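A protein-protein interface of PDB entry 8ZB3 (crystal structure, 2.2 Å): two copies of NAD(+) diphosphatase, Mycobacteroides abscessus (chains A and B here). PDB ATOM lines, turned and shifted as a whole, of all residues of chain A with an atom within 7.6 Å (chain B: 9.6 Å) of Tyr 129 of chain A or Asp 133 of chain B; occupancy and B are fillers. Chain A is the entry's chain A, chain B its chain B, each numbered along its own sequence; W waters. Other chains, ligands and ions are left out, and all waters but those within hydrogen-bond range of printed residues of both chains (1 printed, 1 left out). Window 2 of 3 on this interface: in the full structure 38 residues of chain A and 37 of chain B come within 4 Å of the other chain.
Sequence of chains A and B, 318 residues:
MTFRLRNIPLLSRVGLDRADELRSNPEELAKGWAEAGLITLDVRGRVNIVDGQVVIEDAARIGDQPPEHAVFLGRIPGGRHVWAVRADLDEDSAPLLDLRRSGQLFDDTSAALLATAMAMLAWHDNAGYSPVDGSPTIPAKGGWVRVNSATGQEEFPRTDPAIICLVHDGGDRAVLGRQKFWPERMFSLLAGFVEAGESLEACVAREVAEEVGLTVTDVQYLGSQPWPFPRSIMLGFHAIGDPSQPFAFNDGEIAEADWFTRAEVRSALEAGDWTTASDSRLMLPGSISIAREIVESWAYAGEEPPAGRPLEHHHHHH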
ATOM      1  N   HIS A 124     -13.936 -12.512  -1.191  1.00  0.00           N
ATOM      2  CA  HIS A 124     -13.326 -11.648  -0.191  1.00  0.00           C
ATOM      3  C   HIS A 124     -12.671 -12.470   0.915  1.00  0.00           C
ATOM      4  O   HIS A 124     -11.535 -12.212   1.273  1.00  0.00           O
ATOM      5  CB  HIS A 124     -14.312 -10.620   0.373  1.00  0.00           C
ATOM      6  CG  HIS A 124     -14.497  -9.465  -0.541  1.00  0.00           C
ATOM      7  ND1 HIS A 124     -13.513  -8.516  -0.723  1.00  0.00           N
ATOM      8  CD2 HIS A 124     -15.532  -9.110  -1.334  1.00  0.00           C
ATOM      9  CE1 HIS A 124     -13.939  -7.628  -1.607  1.00  0.00           C
ATOM     10  NE2 HIS A 124     -15.168  -7.981  -2.008  1.00  0.00           N
ATOM     11  N   ASP A 125     -13.385 -13.478   1.410  1.00  0.00           N
ATOM     12  CA  ASP A 125     -12.877 -14.366   2.444  1.00  0.00           C
ATOM     13  C   ASP A 125     -11.564 -15.027   2.022  1.00  0.00           C
ATOM     14  O   ASP A 125     -10.750 -15.330   2.873  1.00  0.00           O
ATOM     15  CB  ASP A 125     -13.892 -15.455   2.796  1.00  0.00           C
ATOM     16  CG  ASP A 125     -15.120 -14.957   3.546  1.00  0.00           C
ATOM     17  OD1 ASP A 125     -15.063 -13.854   4.062  1.00  0.00           O
ATOM     18  OD2 ASP A 125     -16.148 -15.689   3.594  1.00  0.00           O
ATOM     19  N   ASN A 126     -11.358 -15.236   0.721  1.00  0.00           N
ATOM     20  CA  ASN A 126     -10.224 -15.989   0.201  1.00  0.00           C
ATOM     21  C   ASN A 126      -9.244 -15.107  -0.582  1.00  0.00           C
ATOM     22  O   ASN A 126      -8.416 -15.627  -1.334  1.00  0.00           O
ATOM     23  CB  ASN A 126     -10.736 -17.135  -0.688  1.00  0.00           C
ATOM     24  CG  ASN A 126     -11.339 -18.227   0.168  1.00  0.00           C
ATOM     25  OD1 ASN A 126     -10.653 -19.008   0.816  1.00  0.00           O
ATOM     26  ND2 ASN A 126     -12.643 -18.224   0.311  1.00  0.00           N
ATOM     27  N   ALA A 127      -9.352 -13.779  -0.445  1.00  0.00           N
ATOM     28  CA  ALA A 127      -8.539 -12.872  -1.234  1.00  0.00           C
ATOM     29  C   ALA A 127      -7.950 -11.772  -0.347  1.00  0.00           C
ATOM     30  O   ALA A 127      -7.579 -10.715  -0.849  1.00  0.00           O
ATOM     31  CB  ALA A 127      -9.360 -12.294  -2.377  1.00  0.00           C
ATOM     32  N   GLY A 128      -7.830 -12.039   0.957  1.00  0.00           N
ATOM     33  CA  GLY A 128      -7.293 -11.077   1.900  1.00  0.00           C
ATOM     34  C   GLY A 128      -5.830 -10.703   1.643  1.00  0.00           C
ATOM     35  O   GLY A 128      -5.373  -9.691   2.151  1.00  0.00           O
ATOM     36  N   TYR A 129      -5.101 -11.510   0.865  1.00  0.00           N
ATOM     37  CA  TYR A 129      -3.701 -11.246   0.592  1.00  0.00           C
ATOM     38  C   TYR A 129      -3.412 -11.381  -0.906  1.00  0.00           C
ATOM     39  O   TYR A 129      -4.055 -12.166  -1.601  1.00  0.00           O
ATOM     40  CB  TYR A 129      -2.855 -12.239   1.406  1.00  0.00           C
ATOM     41  CG  TYR A 129      -3.055 -12.125   2.910  1.00  0.00           C
ATOM     42  CD1 TYR A 129      -4.160 -12.716   3.522  1.00  0.00           C
ATOM     43  CD2 TYR A 129      -2.192 -11.374   3.714  1.00  0.00           C
ATOM     44  CE1 TYR A 129      -4.387 -12.598   4.886  1.00  0.00           C
ATOM     45  CE2 TYR A 129      -2.437 -11.215   5.073  1.00  0.00           C
ATOM     46  CZ  TYR A 129      -3.515 -11.853   5.663  1.00  0.00           C
ATOM     47  OH  TYR A 129      -3.752 -11.749   7.009  1.00  0.00           O
ATOM     48  N   SER A 130      -2.395 -10.651  -1.370  1.00  0.00           N
ATOM     49  CA  SER A 130      -1.927 -10.744  -2.733  1.00  0.00           C
ATOM     50  C   SER A 130      -1.302 -12.111  -2.966  1.00  0.00           C
ATOM     51  O   SER A 130      -0.433 -12.522  -2.206  1.00  0.00           O
ATOM     52  CB  SER A 130      -0.932  -9.659  -3.065  1.00  0.00           C
ATOM     53  OG  SER A 130      -0.346  -9.862  -4.361  1.00  0.00           O
ATOM     54  N   PRO A 131      -1.723 -12.838  -4.031  1.00  0.00           N
ATOM     55  CA  PRO A 131      -1.034 -14.056  -4.426  1.00  0.00           C
ATOM     56  C   PRO A 131       0.352 -13.758  -4.997  1.00  0.00           C
ATOM     57  O   PRO A 131       1.197 -14.656  -5.079  1.00  0.00           O
ATOM     58  CB  PRO A 131      -1.972 -14.687  -5.475  1.00  0.00           C
ATOM     59  CG  PRO A 131      -2.767 -13.506  -6.044  1.00  0.00           C
ATOM     60  CD  PRO A 131      -2.885 -12.523  -4.894  1.00  0.00           C
ATOM     61  N   VAL A 132       0.578 -12.499  -5.400  1.00  0.00           N
ATOM     62  CA  VAL A 132       1.800 -12.119  -6.086  1.00  0.00           C
ATOM     63  C   VAL A 132       2.923 -11.965  -5.066  1.00  0.00           C
ATOM     64  O   VAL A 132       3.994 -12.521  -5.258  1.00  0.00           O
ATOM     65  CB  VAL A 132       1.625 -10.840  -6.925  1.00  0.00           C
ATOM     66  CG1 VAL A 132       2.877 -10.543  -7.740  1.00  0.00           C
ATOM     67  CG2 VAL A 132       0.415 -10.930  -7.849  1.00  0.00           C
ATOM     68  N   ASP A 133       2.673 -11.225  -3.977  1.00  0.00           N
ATOM     69  CA  ASP A 133       3.742 -10.854  -3.072  1.00  0.00           C
ATOM     70  C   ASP A 133       3.357 -11.040  -1.605  1.00  0.00           C
ATOM     71  O   ASP A 133       4.156 -10.723  -0.732  1.00  0.00           O
ATOM     72  CB  ASP A 133       4.155  -9.409  -3.342  1.00  0.00           C
ATOM     73  CG  ASP A 133       3.084  -8.385  -3.015  1.00  0.00           C
ATOM     74  OD1 ASP A 133       2.132  -8.728  -2.294  1.00  0.00           O
ATOM     75  OD2 ASP A 133       3.196  -7.268  -3.504  1.00  0.00           O
ATOM     76  N   GLY A 134       2.135 -11.499  -1.317  1.00  0.00           N
ATOM     77  CA  GLY A 134       1.750 -11.819   0.048  1.00  0.00           C
ATOM     78  C   GLY A 134       1.245 -10.629   0.863  1.00  0.00           C
ATOM     79  O   GLY A 134       0.816 -10.828   1.991  1.00  0.00           O
ATOM     80  N   SER A 135       1.246  -9.409   0.309  1.00  0.00           N
ATOM     81  CA  SER A 135       0.770  -8.244   1.048  1.00  0.00           C
ATOM     82  C   SER A 135      -0.723  -8.359   1.352  1.00  0.00           C
ATOM     83  O   SER A 135      -1.480  -8.844   0.525  1.00  0.00           O
ATOM     84  CB  SER A 135       1.018  -6.961   0.307  1.00  0.00           C
ATOM     85  OG  SER A 135       2.365  -6.859  -0.109  1.00  0.00           O
ATOM     86  N   PRO A 136      -1.205  -7.864   2.514  1.00  0.00           N
ATOM     87  CA  PRO A 136      -2.644  -7.722   2.738  1.00  0.00           C
ATOM     88  C   PRO A 136      -3.286  -6.874   1.641  1.00  0.00           C
ATOM     89  O   PRO A 136      -2.656  -5.978   1.094  1.00  0.00           O
ATOM     90  CB  PRO A 136      -2.755  -7.036   4.115  1.00  0.00           C
ATOM     91  CG  PRO A 136      -1.419  -7.306   4.795  1.00  0.00           C
ATOM     92  CD  PRO A 136      -0.405  -7.452   3.678  1.00  0.00           C
ATOM     93  N   THR A 137      -4.547  -7.173   1.323  1.00  0.00           N
ATOM     94  CA  THR A 137      -5.302  -6.394   0.355  1.00  0.00           C
ATOM     95  C   THR A 137      -6.475  -5.756   1.083  1.00  0.00           C
ATOM     96  O   THR A 137      -6.945  -6.299   2.073  1.00  0.00           O
ATOM     97  CB  THR A 137      -5.744  -7.255  -0.837  1.00  0.00           C
ATOM     98  OG1 THR A 137      -6.656  -8.245  -0.365  1.00  0.00           O
ATOM     99  CG2 THR A 137      -4.579  -7.926  -1.534  1.00  0.00           C
ATOM    100  N   ILE A 138      -6.950  -4.617   0.567  1.00  0.00           N
ATOM    101  CA  ILE A 138      -8.013  -3.850   1.194  1.00  0.00           C
ATOM    102  C   ILE A 138      -9.127  -3.731   0.164  1.00  0.00           C
ATOM    103  O   ILE A 138      -8.876  -3.362  -0.971  1.00  0.00           O
ATOM    104  CB  ILE A 138      -7.499  -2.465   1.663  1.00  0.00           C
ATOM    105  CG1 ILE A 138      -6.429  -2.607   2.747  1.00  0.00           C
ATOM    106  CG2 ILE A 138      -8.608  -1.566   2.181  1.00  0.00           C
ATOM    107  CD1 ILE A 138      -5.017  -2.325   2.273  1.00  0.00           C
ATOM    108  N   ARG A 146      -9.918  -5.649  -4.617  1.00  0.00           N
ATOM    109  CA  ARG A 146      -9.115  -5.483  -3.416  1.00  0.00           C
ATOM    110  C   ARG A 146      -7.759  -4.932  -3.848  1.00  0.00           C
ATOM    111  O   ARG A 146      -7.222  -5.374  -4.859  1.00  0.00           O
ATOM    112  CB  ARG A 146      -8.992  -6.814  -2.666  1.00  0.00           C
ATOM    113  CG  ARG A 146     -10.325  -7.349  -2.167  1.00  0.00           C
ATOM    114  CD  ARG A 146     -10.169  -8.574  -1.326  1.00  0.00           C
ATOM    115  NE  ARG A 146      -9.506  -8.242  -0.074  1.00  0.00           N
ATOM    116  CZ  ARG A 146     -10.095  -8.150   1.111  1.00  0.00           C
ATOM    117  NH1 ARG A 146     -11.392  -8.320   1.251  1.00  0.00           N
ATOM    118  NH2 ARG A 146      -9.373  -7.876   2.171  1.00  0.00           N
ATOM    119  N   ASN A 148      -3.772  -4.099  -3.243  1.00  0.00           N
ATOM    120  CA  ASN A 148      -2.524  -4.453  -2.577  1.00  0.00           C
ATOM    121  C   ASN A 148      -2.068  -3.258  -1.730  1.00  0.00           C
ATOM    122  O   ASN A 148      -1.816  -2.182  -2.259  1.00  0.00           O
ATOM    123  CB  ASN A 148      -1.466  -4.866  -3.606  1.00  0.00           C
ATOM    124  CG  ASN A 148      -0.193  -5.393  -2.978  1.00  0.00           C
ATOM    125  OD1 ASN A 148       0.372  -4.774  -2.081  1.00  0.00           O
ATOM    126  ND2 ASN A 148       0.249  -6.558  -3.415  1.00  0.00           N
ATOM    127  N   GLU A 155      -6.524  -6.529  -7.243  1.00  0.00           N
ATOM    128  CA  GLU A 155      -6.909  -7.921  -7.413  1.00  0.00           C
ATOM    129  C   GLU A 155      -8.413  -7.986  -7.700  1.00  0.00           C
ATOM    130  O   GLU A 155      -9.202  -7.234  -7.116  1.00  0.00           O
ATOM    131  CB  GLU A 155      -6.596  -8.716  -6.147  1.00  0.00           C
ATOM    132  CG  GLU A 155      -5.110  -8.848  -5.841  1.00  0.00           C
ATOM    133  CD  GLU A 155      -4.289  -9.602  -6.876  1.00  0.00           C
ATOM    134  OE1 GLU A 155      -3.140  -9.180  -7.144  1.00  0.00           O
ATOM    135  OE2 GLU A 155      -4.799 -10.599  -7.442  1.00  0.00           O
ATOM    136  N   ASN B 126       2.790 -15.370 -10.340  1.00  0.00           N
ATOM    137  CA  ASN B 126       1.773 -14.564  -9.678  1.00  0.00           C
ATOM    138  C   ASN B 126       1.018 -15.330  -8.592  1.00  0.00           C
ATOM    139  O   ASN B 126      -0.033 -14.876  -8.149  1.00  0.00           O
ATOM    140  CB  ASN B 126       0.796 -14.027 -10.730  1.00  0.00           C
ATOM    141  CG  ASN B 126       1.448 -12.920 -11.524  1.00  0.00           C
ATOM    142  OD1 ASN B 126       1.570 -11.798 -11.035  1.00  0.00           O
ATOM    143  ND2 ASN B 126       1.956 -13.256 -12.696  1.00  0.00           N
ATOM    144  N   ALA B 127       1.552 -16.477  -8.157  1.00  0.00           N
ATOM    145  CA  ALA B 127       0.856 -17.319  -7.197  1.00  0.00           C
ATOM    146  C   ALA B 127       1.813 -17.779  -6.094  1.00  0.00           C
ATOM    147  O   ALA B 127       1.564 -18.788  -5.450  1.00  0.00           O
ATOM    148  CB  ALA B 127       0.219 -18.494  -7.920  1.00  0.00           C
ATOM    149  N   GLY B 128       2.869 -16.996  -5.841  1.00  0.00           N
ATOM    150  CA  GLY B 128       3.880 -17.363  -4.860  1.00  0.00           C
ATOM    151  C   GLY B 128       3.349 -17.380  -3.430  1.00  0.00           C
ATOM    152  O   GLY B 128       3.974 -17.968  -2.548  1.00  0.00           O
ATOM    153  N   TYR B 129       2.197 -16.739  -3.192  1.00  0.00           N
ATOM    154  CA  TYR B 129       1.624 -16.672  -1.857  1.00  0.00           C
ATOM    155  C   TYR B 129       0.135 -17.017  -1.880  1.00  0.00           C
ATOM    156  O   TYR B 129      -0.545 -16.806  -2.880  1.00  0.00           O
ATOM    157  CB  TYR B 129       1.836 -15.262  -1.314  1.00  0.00           C
ATOM    158  CG  TYR B 129       3.295 -14.853  -1.207  1.00  0.00           C
ATOM    159  CD1 TYR B 129       4.001 -14.423  -2.321  1.00  0.00           C
ATOM    160  CD2 TYR B 129       3.978 -14.955   0.004  1.00  0.00           C
ATOM    161  CE1 TYR B 129       5.341 -14.084  -2.236  1.00  0.00           C
ATOM    162  CE2 TYR B 129       5.303 -14.554   0.115  1.00  0.00           C
ATOM    163  CZ  TYR B 129       5.987 -14.132  -1.008  1.00  0.00           C
ATOM    164  OH  TYR B 129       7.293 -13.758  -0.890  1.00  0.00           O
ATOM    165  N   SER B 130      -0.366 -17.524  -0.751  1.00  0.00           N
ATOM    166  CA  SER B 130      -1.776 -17.809  -0.574  1.00  0.00           C
ATOM    167  C   SER B 130      -2.558 -16.506  -0.564  1.00  0.00           C
ATOM    168  O   SER B 130      -2.223 -15.587   0.182  1.00  0.00           O
ATOM    169  CB  SER B 130      -2.041 -18.575   0.685  1.00  0.00           C
ATOM    170  OG  SER B 130      -3.439 -18.696   0.935  1.00  0.00           O
ATOM    171  N   PRO B 131      -3.618 -16.382  -1.398  1.00  0.00           N
ATOM    172  CA  PRO B 131      -4.531 -15.245  -1.285  1.00  0.00           C
ATOM    173  C   PRO B 131      -5.358 -15.310  -0.005  1.00  0.00           C
ATOM    174  O   PRO B 131      -5.929 -14.313   0.417  1.00  0.00           O
ATOM    175  CB  PRO B 131      -5.376 -15.345  -2.574  1.00  0.00           C
ATOM    176  CG  PRO B 131      -5.339 -16.798  -2.951  1.00  0.00           C
ATOM    177  CD  PRO B 131      -3.983 -17.294  -2.485  1.00  0.00           C
ATOM    178  N   VAL B 132      -5.431 -16.497   0.601  1.00  0.00           N
ATOM    179  CA  VAL B 132      -6.283 -16.725   1.760  1.00  0.00           C
ATOM    180  C   VAL B 132      -5.617 -16.148   3.013  1.00  0.00           C
ATOM    181  O   VAL B 132      -6.239 -15.381   3.754  1.00  0.00           O
ATOM    182  CB  VAL B 132      -6.636 -18.208   1.947  1.00  0.00           C
ATOM    183  CG1 VAL B 132      -7.660 -18.375   3.067  1.00  0.00           C
ATOM    184  CG2 VAL B 132      -7.139 -18.850   0.650  1.00  0.00           C
ATOM    185  N   ASP B 133      -4.343 -16.480   3.235  1.00  0.00           N
ATOM    186  CA  ASP B 133      -3.702 -16.127   4.496  1.00  0.00           C
ATOM    187  C   ASP B 133      -2.305 -15.537   4.299  1.00  0.00           C
ATOM    188  O   ASP B 133      -1.652 -15.223   5.285  1.00  0.00           O
ATOM    189  CB  ASP B 133      -3.639 -17.347   5.405  1.00  0.00           C
ATOM    190  CG  ASP B 133      -2.749 -18.459   4.883  1.00  0.00           C
ATOM    191  OD1 ASP B 133      -1.928 -18.193   3.990  1.00  0.00           O
ATOM    192  OD2 ASP B 133      -2.917 -19.587   5.335  1.00  0.00           O
ATOM    193  N   GLY B 134      -1.831 -15.414   3.055  1.00  0.00           N
ATOM    194  CA  GLY B 134      -0.571 -14.750   2.788  1.00  0.00           C
ATOM    195  C   GLY B 134       0.665 -15.654   2.937  1.00  0.00           C
ATOM    196  O   GLY B 134       1.764 -15.189   2.657  1.00  0.00           O
ATOM    197  N   SER B 135       0.510 -16.927   3.325  1.00  0.00           N
ATOM    198  CA  SER B 135       1.649 -17.830   3.436  1.00  0.00           C
ATOM    199  C   SER B 135       2.299 -18.074   2.077  1.00  0.00           C
ATOM    200  O   SER B 135       1.621 -18.169   1.068  1.00  0.00           O
ATOM    201  CB  SER B 135       1.258 -19.165   4.026  1.00  0.00           C
ATOM    202  OG  SER B 135       0.550 -19.003   5.238  1.00  0.00           O
ATOM    203  N   PRO B 136       3.641 -18.234   2.005  1.00  0.00           N
ATOM    204  CA  PRO B 136       4.284 -18.695   0.779  1.00  0.00           C
ATOM    205  C   PRO B 136       3.700 -20.033   0.330  1.00  0.00           C
ATOM    206  O   PRO B 136       3.280 -20.845   1.155  1.00  0.00           O
ATOM    207  CB  PRO B 136       5.769 -18.845   1.166  1.00  0.00           C
ATOM    208  CG  PRO B 136       5.934 -17.890   2.335  1.00  0.00           C
ATOM    209  CD  PRO B 136       4.611 -17.935   3.076  1.00  0.00           C
ATOM    210  N   THR B 137       3.671 -20.248  -0.990  1.00  0.00           N
ATOM    211  CA  THR B 137       3.206 -21.510  -1.537  1.00  0.00           C
ATOM    212  C   THR B 137       4.378 -22.188  -2.242  1.00  0.00           C
ATOM    213  O   THR B 137       5.290 -21.510  -2.700  1.00  0.00           O
ATOM    214  CB  THR B 137       2.010 -21.306  -2.472  1.00  0.00           C
ATOM    215  OG1 THR B 137       2.432 -20.533  -3.593  1.00  0.00           O
ATOM    216  CG2 THR B 137       0.853 -20.627  -1.779  1.00  0.00           C
ATOM    217  N   VAL B 147       1.246 -25.439  -2.968  1.00  0.00           N
ATOM    218  CA  VAL B 147       0.751 -25.850  -1.668  1.00  0.00           C
ATOM    219  C   VAL B 147       1.079 -24.766  -0.649  1.00  0.00           C
ATOM    220  O   VAL B 147       2.210 -24.300  -0.567  1.00  0.00           O
ATOM    221  CB  VAL B 147       1.335 -27.217  -1.262  1.00  0.00           C
ATOM    222  CG1 VAL B 147       1.030 -27.579   0.178  1.00  0.00           C
ATOM    223  CG2 VAL B 147       0.864 -28.324  -2.199  1.00  0.00           C
ATOM    224  N   ASN B 148       0.061 -24.367   0.117  1.00  0.00           N
ATOM    225  CA  ASN B 148       0.226 -23.450   1.232  1.00  0.00           C
ATOM    226  C   ASN B 148       1.205 -24.073   2.239  1.00  0.00           C
ATOM    227  O   ASN B 148       0.943 -25.147   2.772  1.00  0.00           O
ATOM    228  CB  ASN B 148      -1.126 -23.117   1.856  1.00  0.00           C
ATOM    229  CG  ASN B 148      -1.034 -22.061   2.947  1.00  0.00           C
ATOM    230  OD1 ASN B 148      -0.208 -22.137   3.845  1.00  0.00           O
ATOM    231  ND2 ASN B 148      -1.869 -21.053   2.892  1.00  0.00           N
ATOM    232  N   SER B 149       2.336 -23.404   2.472  1.00  0.00           N
ATOM    233  CA  SER B 149       3.387 -23.941   3.330  1.00  0.00           C
ATOM    234  C   SER B 149       2.899 -24.101   4.772  1.00  0.00           C
ATOM    235  O   SER B 149       3.323 -25.026   5.457  1.00  0.00           O
ATOM    236  CB  SER B 149       4.636 -23.096   3.262  1.00  0.00           C
ATOM    237  OG  SER B 149       4.364 -21.753   3.617  1.00  0.00           O
ATOM    238  N   ALA B 150       1.968 -23.248   5.209  1.00  0.00           N
ATOM    239  CA  ALA B 150       1.431 -23.306   6.560  1.00  0.00           C
ATOM    240  C   ALA B 150       0.306 -24.336   6.684  1.00  0.00           C
ATOM    241  O   ALA B 150       0.277 -25.081   7.657  1.00  0.00           O
ATOM    242  CB  ALA B 150       0.963 -21.936   6.994  1.00  0.00           C
ATOM    243  N   THR B 151      -0.639 -24.377   5.730  1.00  0.00           N
ATOM    244  CA  THR B 151      -1.867 -25.127   5.950  1.00  0.00           C
ATOM    245  C   THR B 151      -1.955 -26.373   5.078  1.00  0.00           C
ATOM    246  O   THR B 151      -2.838 -27.203   5.301  1.00  0.00           O
ATOM    247  CB  THR B 151      -3.123 -24.299   5.662  1.00  0.00           C
ATOM    248  OG1 THR B 151      -3.215 -24.090   4.245  1.00  0.00           O
ATOM    249  CG2 THR B 151      -3.141 -22.992   6.423  1.00  0.00           C
ATOM    250  N   GLY B 152      -1.102 -26.492   4.054  1.00  0.00           N
ATOM    251  CA  GLY B 152      -1.222 -27.613   3.135  1.00  0.00           C
ATOM    252  C   GLY B 152      -2.329 -27.444   2.088  1.00  0.00           C
ATOM    253  O   GLY B 152      -2.507 -28.319   1.246  1.00  0.00           O
ATOM    254  N   GLN B 153      -3.056 -26.321   2.110  1.00  0.00           N
ATOM    255  CA  GLN B 153      -4.120 -26.075   1.144  1.00  0.00           C
ATOM    256  C   GLN B 153      -3.514 -25.881  -0.250  1.00  0.00           C
ATOM    257  O   GLN B 153      -2.527 -25.167  -0.419  1.00  0.00           O
ATOM    258  CB  GLN B 153      -4.930 -24.863   1.607  1.00  0.00           C
ATOM    259  CG  GLN B 153      -6.021 -24.408   0.637  1.00  0.00           C
ATOM    260  CD  GLN B 153      -6.809 -23.222   1.164  1.00  0.00           C
ATOM    261  OE1 GLN B 153      -6.271 -22.248   1.698  1.00  0.00           O
ATOM    262  NE2 GLN B 153      -8.118 -23.305   1.048  1.00  0.00           N
ATOM    263  N   GLU B 155      -3.459 -24.451  -4.030  1.00  0.00           N
ATOM    264  CA  GLU B 155      -3.874 -23.408  -4.959  1.00  0.00           C
ATOM    265  C   GLU B 155      -3.704 -23.935  -6.392  1.00  0.00           C
ATOM    266  O   GLU B 155      -2.732 -24.650  -6.708  1.00  0.00           O
ATOM    267  CB  GLU B 155      -3.017 -22.157  -4.783  1.00  0.00           C
ATOM    268  CG  GLU B 155      -3.170 -21.472  -3.429  1.00  0.00           C
ATOM    269  CD  GLU B 155      -4.567 -20.959  -3.082  1.00  0.00           C
ATOM    270  OE1 GLU B 155      -4.943 -21.093  -1.914  1.00  0.00           O
ATOM    271  OE2 GLU B 155      -5.266 -20.455  -3.991  1.00  0.00           O
ATOM    272  N   ARG B 158      -4.984 -20.270 -12.485  1.00  0.00           N
ATOM    273  CA  ARG B 158      -6.101 -19.377 -12.710  1.00  0.00           C
ATOM    274  C   ARG B 158      -6.207 -19.016 -14.184  1.00  0.00           C
ATOM    275  O   ARG B 158      -5.232 -18.553 -14.778  1.00  0.00           O
ATOM    276  CB  ARG B 158      -5.903 -18.098 -11.895  1.00  0.00           C
ATOM    277  CG  ARG B 158      -7.056 -17.134 -12.071  1.00  0.00           C
ATOM    278  CD  ARG B 158      -6.862 -15.984 -11.131  1.00  0.00           C
ATOM    279  NE  ARG B 158      -7.922 -15.015 -11.293  1.00  0.00           N
ATOM    280  CZ  ARG B 158      -8.281 -14.150 -10.373  1.00  0.00           C
ATOM    281  NH1 ARG B 158      -7.627 -14.086  -9.226  1.00  0.00           N
ATOM    282  NH2 ARG B 158      -9.319 -13.365 -10.596  1.00  0.00           N
HETATM  283  O   HOH W   1       4.344 -14.509  -6.700  1.00  0.00           O
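The backbone NH (N) of Gly 128 of chain A sits at hydrogen-bond distance from the backbone carbonyl oxygen (O) of Pro 131 of chain B.
O of Pro 131 of chain B lies within hydrogen-bond range of N of Tyr 129 of chain A (3.0 Å).
N of Gly 128 of chain B is in hydrogen-bond range of O of Pro 131 of chain A, at 3.0 Å.
O of Pro 131 of chain A is in hydrogen-bond range of N of Tyr 129 of chain B.
The backbone carbonyl oxygen (O) of Asn 126 of chain A sits close to the backbone carbonyl oxygen (O) of Pro 131 of chain B.
The backbone carbonyl oxygen of Pro 131 of chain A sits close to the backbone carbonyl oxygen of Asn 126 of chain B, 3.3 Å away.
OG1 of Thr 137 of chain A is in hydrogen-bond range of O of Ala 127 of chain A (2.7 Å).
The backbone carbonyl oxygen (O) of Ala 127 of chain A lies within hydrogen-bond range of the guanidinium group (NE) of Arg 146 of chain A, at 3.2 Å.
The backbone carbonyl oxygen (O) of Gly 128 of chain A is in hydrogen-bond range of the backbone NH (N) of Thr 137 of chain A (2.8 Å).
OG of Ser 130 of chain A sits at hydrogen-bond distance from N of Val 132 of chain A, 3.0 Å away.
N of Ser 130 of chain A is in hydrogen-bond range of O of Ser 135 of chain A.
OD2 of Asp 133 of chain A sits at hydrogen-bond distance from ND2 of Asn 148 of chain A, at 3.0 Å.
Among the printed residues, pairs that only touch across the chains: Asn 126 of chain A with Val 132 of chain B (3.5 Å), Ala 127 of chain A with Pro 131 of chain B (3.3 Å), Tyr 129 of chain A with Ser 130 of chain B (3.6 Å), Tyr 129 of chain A with Val 132 of chain B (3.4 Å), Tyr 129 of chain A with Asp 133 of chain B (3.5 Å), Tyr 129 of chain A with Gly 134 of chain B (3.5 Å), Ser 130 of chain A with Tyr 129 of chain B (3.7 Å), Pro 131 of chain A with Ala 127 of chain B (3.3 Å), Val 132 of chain A with Asn 126 of chain B (3.5 Å), Val 132 of chain A with Tyr 129 of chain B (3.5 Å), Asp 133 of chain A with Tyr 129 of chain B (3.5 Å) and Gly 134 of chain A with Tyr 129 of chain B (3.6 Å).
Of chain B, only Ser 130, Pro 131, Val 132, Asp 133 and Gly 134 come within 4 Å of Tyr 129 of chain A.
Asp 133 of chain B touches one residue of chain A.
Gly 128 of chain A touches just one residue of chain B: Pro 131.
Of the printed residues of chain A, Asn 126 of chain B touches Pro 131 (3.3 Å) and Val 132 (3.5 Å).
Of the printed residues of chain A, Pro 131 of chain B touches Asn 126 (3.3 Å), Ala 127 (3.3 Å), Gly 128 (3.0 Å) and Tyr 129 (3.0 Å).
Of the printed residues of chain A, Gly 128 of chain B touches Pro 131 (3.0 Å).
Printed residues of chain A within 4 Å of Ala 127 of chain B: Pro 131.
The nearest printed residue of chain A that does not touch Gly 128 of chain B is Val 132 of chain A (4.7 Å).
Hydrophobic or aromatic side chains of chain A that line the printed part of chain B: Tyr 129, Pro 131 and Val 132.
Asn 126 of chain A touches Pro 131 of chain B, and with the chains exchanged Pro 131 of chain A touches Asn 126 of chain B.
Gly 128 of chain A touches Pro 131 of chain B, and with the chains exchanged Pro 131 of chain A touches Gly 128 of chain B.
Tyr 129 of chain A touches Ser 130 of chain B, and with the chains exchanged Ser 130 of chain A touches Tyr 129 of chain B.
Tyr 129 of chain A touches Val 132 of chain B, and with the chains exchanged Val 132 of chain A touches Tyr 129 of chain B.
Of the 18 pairs that touch across the chains among the printed residues, 18 have their exchanged pair printed and touching as well.
Water W1 bridges the backbone carbonyl oxygen of Val 132 of chain A and the backbone NH of Gly 128 of chain B.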
